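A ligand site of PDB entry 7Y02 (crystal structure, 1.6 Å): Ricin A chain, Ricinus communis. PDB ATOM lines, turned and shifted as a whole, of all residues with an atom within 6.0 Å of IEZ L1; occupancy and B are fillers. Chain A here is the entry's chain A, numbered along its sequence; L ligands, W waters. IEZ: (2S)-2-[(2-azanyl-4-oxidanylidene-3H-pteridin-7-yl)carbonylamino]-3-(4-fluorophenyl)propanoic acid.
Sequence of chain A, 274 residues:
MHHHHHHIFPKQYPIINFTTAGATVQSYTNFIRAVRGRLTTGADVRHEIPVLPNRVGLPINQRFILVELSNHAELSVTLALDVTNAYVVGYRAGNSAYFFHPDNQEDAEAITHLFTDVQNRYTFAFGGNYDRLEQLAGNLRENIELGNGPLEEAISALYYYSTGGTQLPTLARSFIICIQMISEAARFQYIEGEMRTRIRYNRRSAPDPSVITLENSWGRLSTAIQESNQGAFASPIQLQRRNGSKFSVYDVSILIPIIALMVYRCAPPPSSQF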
ATOM      1  N   ASN A  85      19.614   7.640 -20.255  1.00  0.00           N
ATOM      2  CA  ASN A  85      20.653   8.686 -20.302  1.00  0.00           C
ATOM      3  C   ASN A  85      21.928   8.285 -21.041  1.00  0.00           C
ATOM      4  O   ASN A  85      22.861   9.086 -21.139  1.00  0.00           O
ATOM      5  CB  ASN A  85      20.981   9.181 -18.887  1.00  0.00           C
ATOM      6  CG  ASN A  85      21.385   8.059 -17.952  1.00  0.00           C
ATOM      7  OD1 ASN A  85      21.660   6.936 -18.379  1.00  0.00           O
ATOM      8  ND2 ASN A  85      21.417   8.356 -16.662  1.00  0.00           N
ATOM      9  N   ALA A  86      21.941   7.061 -21.589  1.00  0.00           N
ATOM     10  CA  ALA A  86      23.119   6.449 -22.248  1.00  0.00           C
ATOM     11  C   ALA A  86      24.329   6.246 -21.313  1.00  0.00           C
ATOM     12  O   ALA A  86      25.442   5.992 -21.765  1.00  0.00           O
ATOM     13  CB  ALA A  86      23.495   7.194 -23.534  1.00  0.00           C
ATOM     14  N   TYR A  87      24.085   6.315 -19.994  1.00  0.00           N
ATOM     15  CA  TYR A  87      25.148   6.198 -18.989  1.00  0.00           C
ATOM     16  C   TYR A  87      25.710   4.779 -18.946  1.00  0.00           C
ATOM     17  O   TYR A  87      24.957   3.803 -18.918  1.00  0.00           O
ATOM     18  CB  TYR A  87      24.581   6.599 -17.625  1.00  0.00           C
ATOM     19  CG  TYR A  87      25.588   6.923 -16.560  1.00  0.00           C
ATOM     20  CD1 TYR A  87      26.102   5.904 -15.741  1.00  0.00           C
ATOM     21  CD2 TYR A  87      26.005   8.232 -16.331  1.00  0.00           C
ATOM     22  CE1 TYR A  87      27.031   6.191 -14.749  1.00  0.00           C
ATOM     23  CE2 TYR A  87      26.923   8.535 -15.323  1.00  0.00           C
ATOM     24  CZ  TYR A  87      27.423   7.505 -14.542  1.00  0.00           C
ATOM     25  OH  TYR A  87      28.335   7.780 -13.555  1.00  0.00           O
ATOM     26  N   VAL A  88      27.041   4.679 -18.964  1.00  0.00           N
ATOM     27  CA  VAL A  88      27.727   3.388 -18.850  1.00  0.00           C
ATOM     28  C   VAL A  88      27.742   3.043 -17.367  1.00  0.00           C
ATOM     29  O   VAL A  88      28.436   3.689 -16.578  1.00  0.00           O
ATOM     30  CB  VAL A  88      29.163   3.441 -19.429  1.00  0.00           C
ATOM     31  CG1 VAL A  88      29.869   2.098 -19.269  1.00  0.00           C
ATOM     32  CG2 VAL A  88      29.154   3.840 -20.906  1.00  0.00           C
ATOM     33  N   VAL A  89      26.974   2.030 -16.991  1.00  0.00           N
ATOM     34  CA  VAL A  89      26.787   1.682 -15.571  1.00  0.00           C
ATOM     35  C   VAL A  89      27.794   0.643 -15.077  1.00  0.00           C
ATOM     36  O   VAL A  89      28.004   0.490 -13.871  1.00  0.00           O
ATOM     37  CB  VAL A  89      25.335   1.239 -15.229  1.00  0.00           C
ATOM     38  CG1 VAL A  89      24.335   2.336 -15.584  1.00  0.00           C
ATOM     39  CG2 VAL A  89      24.953  -0.061 -15.935  1.00  0.00           C
ATOM     40  N   PHE A 100      29.870   0.691 -11.471  1.00  0.00           N
ATOM     41  CA  PHE A 100      30.127   1.932 -10.746  1.00  0.00           C
ATOM     42  C   PHE A 100      29.185   2.046  -9.541  1.00  0.00           C
ATOM     43  O   PHE A 100      28.089   1.482  -9.559  1.00  0.00           O
ATOM     44  CB  PHE A 100      29.951   3.152 -11.651  1.00  0.00           C
ATOM     45  CG  PHE A 100      30.918   3.201 -12.797  1.00  0.00           C
ATOM     46  CD1 PHE A 100      32.288   3.290 -12.568  1.00  0.00           C
ATOM     47  CD2 PHE A 100      30.451   3.168 -14.114  1.00  0.00           C
ATOM     48  CE1 PHE A 100      33.186   3.334 -13.634  1.00  0.00           C
ATOM     49  CE2 PHE A 100      31.341   3.217 -15.184  1.00  0.00           C
ATOM     50  CZ  PHE A 100      32.710   3.293 -14.943  1.00  0.00           C
ATOM     51  N   GLY A 128      30.820   6.739 -11.392  1.00  0.00           N
ATOM     52  CA  GLY A 128      31.360   6.737 -12.757  1.00  0.00           C
ATOM     53  C   GLY A 128      31.341   8.036 -13.539  1.00  0.00           C
ATOM     54  O   GLY A 128      31.599   8.014 -14.747  1.00  0.00           O
ATOM     55  N   ASN A 129      31.049   9.162 -12.890  1.00  0.00           N
ATOM     56  CA  ASN A 129      31.103  10.475 -13.567  1.00  0.00           C
ATOM     57  C   ASN A 129      32.536  10.853 -13.953  1.00  0.00           C
ATOM     58  O   ASN A 129      33.498  10.348 -13.351  1.00  0.00           O
ATOM     59  CB  ASN A 129      30.497  11.578 -12.699  1.00  0.00           C
ATOM     60  CG  ASN A 129      28.995  11.412 -12.473  1.00  0.00           C
ATOM     61  OD1 ASN A 129      28.341  10.542 -13.058  1.00  0.00           O
ATOM     62  ND2 ASN A 129      28.443  12.266 -11.622  1.00  0.00           N
ATOM     63  N   TYR A 130      32.675  11.739 -14.940  1.00  0.00           N
ATOM     64  CA  TYR A 130      33.994  12.184 -15.425  1.00  0.00           C
ATOM     65  C   TYR A 130      34.883  12.709 -14.301  1.00  0.00           C
ATOM     66  O   TYR A 130      36.054  12.341 -14.237  1.00  0.00           O
ATOM     67  CB  TYR A 130      33.898  13.243 -16.519  1.00  0.00           C
ATOM     68  CG  TYR A 130      33.375  12.759 -17.864  1.00  0.00           C
ATOM     69  CD1 TYR A 130      33.782  11.530 -18.410  1.00  0.00           C
ATOM     70  CD2 TYR A 130      32.492  13.549 -18.595  1.00  0.00           C
ATOM     71  CE1 TYR A 130      33.300  11.112 -19.647  1.00  0.00           C
ATOM     72  CE2 TYR A 130      32.007  13.144 -19.834  1.00  0.00           C
ATOM     73  CZ  TYR A 130      32.410  11.913 -20.349  1.00  0.00           C
ATOM     74  OH  TYR A 130      31.930  11.515 -21.565  1.00  0.00           O
ATOM     75  N   ASP A 131      34.324  13.539 -13.417  1.00  0.00           N
ATOM     76  CA  ASP A 131      35.100  14.131 -12.315  1.00  0.00           C
ATOM     77  C   ASP A 131      35.841  13.083 -11.474  1.00  0.00           C
ATOM     78  O   ASP A 131      37.053  13.198 -11.282  1.00  0.00           O
ATOM     79  CB  ASP A 131      34.276  15.115 -11.449  1.00  0.00           C
ATOM     80  CG  ASP A 131      32.965  14.521 -10.912  1.00  0.00           C
ATOM     81  OD1 ASP A 131      32.765  13.282 -10.861  1.00  0.00           O
ATOM     82  OD2 ASP A 131      32.101  15.333 -10.502  1.00  0.00           O
ATOM     83  N   LEU A 133      36.351   9.870 -12.381  1.00  0.00           N
ATOM     84  CA  LEU A 133      37.221   9.079 -13.248  1.00  0.00           C
ATOM     85  C   LEU A 133      38.512   9.811 -13.591  1.00  0.00           C
ATOM     86  O   LEU A 133      39.579   9.183 -13.652  1.00  0.00           O
ATOM     87  CB  LEU A 133      36.473   8.631 -14.507  1.00  0.00           C
ATOM     88  CG  LEU A 133      35.348   7.606 -14.334  1.00  0.00           C
ATOM     89  CD1 LEU A 133      34.754   7.280 -15.694  1.00  0.00           C
ATOM     90  CD2 LEU A 133      35.785   6.311 -13.639  1.00  0.00           C
ATOM     91  N   ARG A 141      39.983  14.867 -19.215  1.00  0.00           N
ATOM     92  CA  ARG A 141      39.572  14.519 -20.583  1.00  0.00           C
ATOM     93  C   ARG A 141      40.384  15.250 -21.651  1.00  0.00           C
ATOM     94  O   ARG A 141      40.757  14.646 -22.649  1.00  0.00           O
ATOM     95  CB  ARG A 141      38.083  14.808 -20.783  1.00  0.00           C
ATOM     96  CG  ARG A 141      37.144  13.772 -20.193  1.00  0.00           C
ATOM     97  CD  ARG A 141      35.715  14.286 -20.251  1.00  0.00           C
ATOM     98  NE  ARG A 141      35.452  15.258 -19.181  1.00  0.00           N
ATOM     99  CZ  ARG A 141      34.512  16.196 -19.210  1.00  0.00           C
ATOM    100  NH1 ARG A 141      33.695  16.318 -20.266  1.00  0.00           N
ATOM    101  NH2 ARG A 141      34.352  17.009 -18.167  1.00  0.00           N
ATOM    102  N   ILE A 179      33.430   5.797 -22.753  1.00  0.00           N
ATOM    103  CA  ILE A 179      32.257   6.662 -22.534  1.00  0.00           C
ATOM    104  C   ILE A 179      32.139   7.703 -23.657  1.00  0.00           C
ATOM    105  O   ILE A 179      31.063   7.907 -24.209  1.00  0.00           O
ATOM    106  CB  ILE A 179      32.272   7.315 -21.138  1.00  0.00           C
ATOM    107  CG1 ILE A 179      32.110   6.253 -20.044  1.00  0.00           C
ATOM    108  CG2 ILE A 179      31.188   8.386 -21.013  1.00  0.00           C
ATOM    109  CD1 ILE A 179      32.648   6.683 -18.697  1.00  0.00           C
ATOM    110  N   SER A 183      28.976   6.584 -25.685  1.00  0.00           N
ATOM    111  CA  SER A 183      27.850   7.371 -25.165  1.00  0.00           C
ATOM    112  C   SER A 183      27.808   8.811 -25.689  1.00  0.00           C
ATOM    113  O   SER A 183      26.753   9.267 -26.139  1.00  0.00           O
ATOM    114  CB  SER A 183      27.834   7.339 -23.631  1.00  0.00           C
ATOM    115  OG  SER A 183      27.720   5.988 -23.194  1.00  0.00           O
ATOM    116  N   GLU A 184      28.931   9.531 -25.654  1.00  0.00           N
ATOM    117  CA  GLU A 184      28.940  10.905 -26.160  1.00  0.00           C
ATOM    118  C   GLU A 184      28.718  10.975 -27.657  1.00  0.00           C
ATOM    119  O   GLU A 184      28.017  11.873 -28.148  1.00  0.00           O
ATOM    120  CB  GLU A 184      30.209  11.667 -25.763  1.00  0.00           C
ATOM    121  CG  GLU A 184      30.478  11.745 -24.273  1.00  0.00           C
ATOM    122  CD  GLU A 184      29.489  12.588 -23.462  1.00  0.00           C
ATOM    123  OE1 GLU A 184      28.460  13.063 -23.991  1.00  0.00           O
ATOM    124  OE2 GLU A 184      29.754  12.763 -22.257  1.00  0.00           O
ATOM    125  N   ARG A 187      25.086  10.567 -28.193  1.00  0.00           N
ATOM    126  CA  ARG A 187      24.372  11.783 -27.798  1.00  0.00           C
ATOM    127  C   ARG A 187      24.514  12.916 -28.810  1.00  0.00           C
ATOM    128  O   ARG A 187      23.567  13.684 -29.020  1.00  0.00           O
ATOM    129  CB  ARG A 187      24.858  12.263 -26.435  1.00  0.00           C
ATOM    130  CG  ARG A 187      24.463  11.373 -25.272  1.00  0.00           C
ATOM    131  CD  ARG A 187      25.236  11.786 -24.032  1.00  0.00           C
ATOM    132  NE  ARG A 187      24.980  10.868 -22.927  1.00  0.00           N
ATOM    133  CZ  ARG A 187      25.897  10.491 -22.042  1.00  0.00           C
ATOM    134  NH1 ARG A 187      27.142  10.949 -22.124  1.00  0.00           N
ATOM    135  NH2 ARG A 187      25.566   9.658 -21.065  1.00  0.00           N
ATOM    136  N   GLU A 215      29.994  17.972 -24.152  1.00  0.00           N
ATOM    137  CA  GLU A 215      29.815  16.920 -23.143  1.00  0.00           C
ATOM    138  C   GLU A 215      29.298  17.518 -21.833  1.00  0.00           C
ATOM    139  O   GLU A 215      28.321  17.029 -21.265  1.00  0.00           O
ATOM    140  CB  GLU A 215      31.105  16.167 -22.878  1.00  0.00           C
ATOM    141  CG  GLU A 215      31.613  15.374 -24.082  1.00  0.00           C
ATOM    142  CD  GLU A 215      32.981  14.768 -23.865  1.00  0.00           C
ATOM    143  OE1 GLU A 215      33.621  15.031 -22.839  1.00  0.00           O
ATOM    144  OE2 GLU A 215      33.433  14.024 -24.761  1.00  0.00           O
ATOM    145  N   ASN A 216      29.950  18.595 -21.393  1.00  0.00           N
ATOM    146  CA  ASN A 216      29.583  19.268 -20.160  1.00  0.00           C
ATOM    147  C   ASN A 216      28.198  19.890 -20.167  1.00  0.00           C
ATOM    148  O   ASN A 216      27.601  20.069 -19.108  1.00  0.00           O
ATOM    149  CB  ASN A 216      30.628  20.312 -19.779  1.00  0.00           C
ATOM    150  CG  ASN A 216      31.970  19.705 -19.431  1.00  0.00           C
ATOM    151  OD1 ASN A 216      32.085  18.511 -19.154  1.00  0.00           O
ATOM    152  ND2 ASN A 216      33.009  20.537 -19.444  1.00  0.00           N
ATOM    153  N   SER A 217      27.701  20.206 -21.359  1.00  0.00           N
ATOM    154  CA  SER A 217      26.453  20.944 -21.518  1.00  0.00           C
ATOM    155  C   SER A 217      25.257  20.080 -21.906  1.00  0.00           C
ATOM    156  O   SER A 217      24.169  20.616 -22.106  1.00  0.00           O
ATOM    157  CB  SER A 217      26.624  22.083 -22.530  1.00  0.00           C
ATOM    158  OG  SER A 217      27.652  22.982 -22.119  1.00  0.00           O
HETATM  159  CD1 IEZ L   1      27.867  18.765 -16.378  1.00  0.00           C
HETATM  160  CE1 IEZ L   1      27.964  20.003 -15.720  1.00  0.00           C
HETATM  161  CZ  IEZ L   1      29.219  20.560 -15.459  1.00  0.00           C
HETATM  162  FAX IEZ L   1      29.306  21.790 -14.793  1.00  0.00           F
HETATM  163  CE2 IEZ L   1      30.382  19.886 -15.855  1.00  0.00           C
HETATM  164  CD2 IEZ L   1      30.291  18.656 -16.512  1.00  0.00           C
HETATM  165  CG  IEZ L   1      29.031  18.091 -16.774  1.00  0.00           C
HETATM  166  CB  IEZ L   1      28.906  16.741 -17.519  1.00  0.00           C
HETATM  167  CA  IEZ L   1      29.308  15.567 -16.622  1.00  0.00           C
HETATM  168  C   IEZ L   1      28.434  15.563 -15.343  1.00  0.00           C
HETATM  169  OXT IEZ L   1      27.303  15.036 -15.402  1.00  0.00           O
HETATM  170  O   IEZ L   1      28.920  16.100 -14.325  1.00  0.00           O
HETATM  171  N   IEZ L   1      29.140  14.273 -17.337  1.00  0.00           N
HETATM  172  CAL IEZ L   1      29.811  13.164 -16.956  1.00  0.00           C
HETATM  173  OAQ IEZ L   1      30.516  13.171 -15.950  1.00  0.00           O
HETATM  174  C7  IEZ L   1      29.468  11.957 -17.568  1.00  0.00           C
HETATM  175  N8  IEZ L   1      29.830  10.798 -16.962  1.00  0.00           N
HETATM  176  C8A IEZ L   1      29.485   9.599 -17.457  1.00  0.00           C
HETATM  177  N1  IEZ L   1      29.885   8.484 -16.818  1.00  0.00           N
HETATM  178  C2  IEZ L   1      29.567   7.250 -17.254  1.00  0.00           C
HETATM  179  N2  IEZ L   1      29.967   6.177 -16.587  1.00  0.00           N
HETATM  180  N3  IEZ L   1      28.811   7.084 -18.415  1.00  0.00           N
HETATM  181  C4  IEZ L   1      28.376   8.226 -19.104  1.00  0.00           C
HETATM  182  O4  IEZ L   1      27.717   8.068 -20.139  1.00  0.00           O
HETATM  183  C4A IEZ L   1      28.723   9.496 -18.628  1.00  0.00           C
HETATM  184  N5  IEZ L   1      28.341  10.623 -19.260  1.00  0.00           N
HETATM  185  C6  IEZ L   1      28.696  11.882 -18.736  1.00  0.00           C
HETATM  186  CD1 IEZ L   2      23.156  14.379 -17.437  1.00  0.00           C
HETATM  187  CE1 IEZ L   2      24.349  14.496 -18.146  1.00  0.00           C
HETATM  188  CZ  IEZ L   2      25.020  13.344 -18.578  1.00  0.00           C
HETATM  189  FAX IEZ L   2      26.130  13.481 -19.249  1.00  0.00           F
HETATM  190  CE2 IEZ L   2      24.508  12.070 -18.306  1.00  0.00           C
HETATM  191  CD2 IEZ L   2      23.298  11.950 -17.592  1.00  0.00           C
HETATM  192  CG  IEZ L   2      22.632  13.110 -17.159  1.00  0.00           C
HETATM  193  CB  IEZ L   2      21.326  13.001 -16.367  1.00  0.00           C
HETATM  194  CA  IEZ L   2      21.665  13.000 -14.861  1.00  0.00           C
HETATM  195  C   IEZ L   2      20.459  13.401 -13.973  1.00  0.00           C
HETATM  196  OXT IEZ L   2      19.845  14.453 -14.259  1.00  0.00           O
HETATM  197  O   IEZ L   2      20.210  12.659 -12.994  1.00  0.00           O
HETATM  198  N   IEZ L   2      22.201  11.676 -14.458  1.00  0.00           N
HETATM  199  CAL IEZ L   2      23.483  11.472 -14.092  1.00  0.00           C
HETATM  200  OAQ IEZ L   2      24.318  12.375 -14.014  1.00  0.00           O
HETATM  201  C7  IEZ L   2      23.774  10.158 -13.674  1.00  0.00           C
HETATM  202  N8  IEZ L   2      23.075   9.102 -14.148  1.00  0.00           N
HETATM  203  C8A IEZ L   2      23.317   7.839 -13.723  1.00  0.00           C
HETATM  204  N1  IEZ L   2      22.599   6.809 -14.229  1.00  0.00           N
HETATM  205  C2  IEZ L   2      22.816   5.541 -13.836  1.00  0.00           C
HETATM  206  N2  IEZ L   2      22.086   4.554 -14.341  1.00  0.00           N
HETATM  207  N3  IEZ L   2      23.799   5.244 -12.877  1.00  0.00           N
HETATM  208  C4  IEZ L   2      24.553   6.295 -12.336  1.00  0.00           C
HETATM  209  O4  IEZ L   2      25.410   6.029 -11.499  1.00  0.00           O
HETATM  210  C4A IEZ L   2      24.315   7.603 -12.764  1.00  0.00           C
HETATM  211  N5  IEZ L   2      25.028   8.637 -12.271  1.00  0.00           N
HETATM  212  C6  IEZ L   2      24.770   9.946 -12.708  1.00  0.00           C
HETATM  213  O   HOH W   1      28.685  14.478 -20.408  1.00  0.00           O
HETATM  214  O   HOH W   2      31.578  14.742 -13.843  1.00  0.00           O
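O of Ile 179 is in hydrogen-bond range of N of Glu 184 (3.0 Å).
The backbone NH (N) of Tyr 87 sits at hydrogen-bond distance from the side-chain amide oxygen (OD1) of Asn 85, at 3.0 Å.
The guanidinium group of Arg 141 is in salt-bridge range of the side-chain carboxylate of Glu 215.
OH of Tyr 87 is in hydrogen-bond range of OD1 of Asn 129 (2.8 Å).
The guanidinium group of Arg 187 sits at hydrogen-bond distance from the backbone carbonyl oxygen of Asn 85 (2.8 Å).
OH of Tyr 87 sits close to N of Gly 128 (3.5 Å).
OG of Ser 183 is in hydrogen-bond range of O of Ala 86, at 2.7 Å.
The side-chain amide oxygen of Asn 216 sits at hydrogen-bond distance from the guanidinium group of Arg 141, 2.9 Å away.
ND2 of Asn 85 is in hydrogen-bond range of N8 of IEZ L2 (3.1 Å).
OAQ of IEZ L1 lies within hydrogen-bond range of N of Tyr 130, 2.8 Å away.
N2 of IEZ L1 is in hydrogen-bond range of O of Val 88 (2.9 Å).
The backbone carbonyl oxygen of Gly 128 lies within hydrogen-bond range of a nitrogen (N2) of IEZ L1, 3.1 Å away.
NH2 of Arg 187 sits at hydrogen-bond distance from O4 of IEZ L1 (2.8 Å).
Water W2 lies within hydrogen-bond range of an oxygen (OAQ) of IEZ L1 (2.8 Å), the backbone NH (N) of Asp 131 (3.0 Å) and the backbone NH (N) of Tyr 130 (3.4 Å).
Water W1 lies within hydrogen-bond range of the backbone carbonyl oxygen of Glu 215 (2.7 Å), the side-chain carboxylate of Glu 184 (2.7 Å) and a nitrogen (N) of IEZ L1 (3.1 Å).
O of Ala 86 lies close to O4 of IEZ L1, 3.5 Å away.
CE2 of Tyr 87 touches N1 of IEZ L1, 3.3 Å away.
CE2 of Phe 100 touches N2 of IEZ L1 (3.6 Å).
Asn 129 touches IEZ L1.
CG2 of Ile 179 touches C4 of IEZ L1 (3.4 Å).
Ser 183 touches IEZ L1.
OE2 of Glu 184 touches C6 of IEZ L1 (3.8 Å).
O of Glu 215 touches CB of IEZ L1, 3.8 Å away.
O of Asn 216 touches CD1 of IEZ L1, at 3.0 Å.
Hydrophobic or aromatic side chains within 4 Å of IEZ L1: Tyr 87, Val 88, Phe 100, Tyr 130 and Ile 179.
13 residues have an atom within 4 Å of IEZ L1: Ala 86, Tyr 87, Val 88, Phe 100, Gly 128, Asn 129, Tyr 130, Ile 179, Ser 183, Glu 184, Arg 187, Glu 215 and Asn 216.
The nearest printed residue that does not touch IEZ L1 is Asp 131 (4.6 Å).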
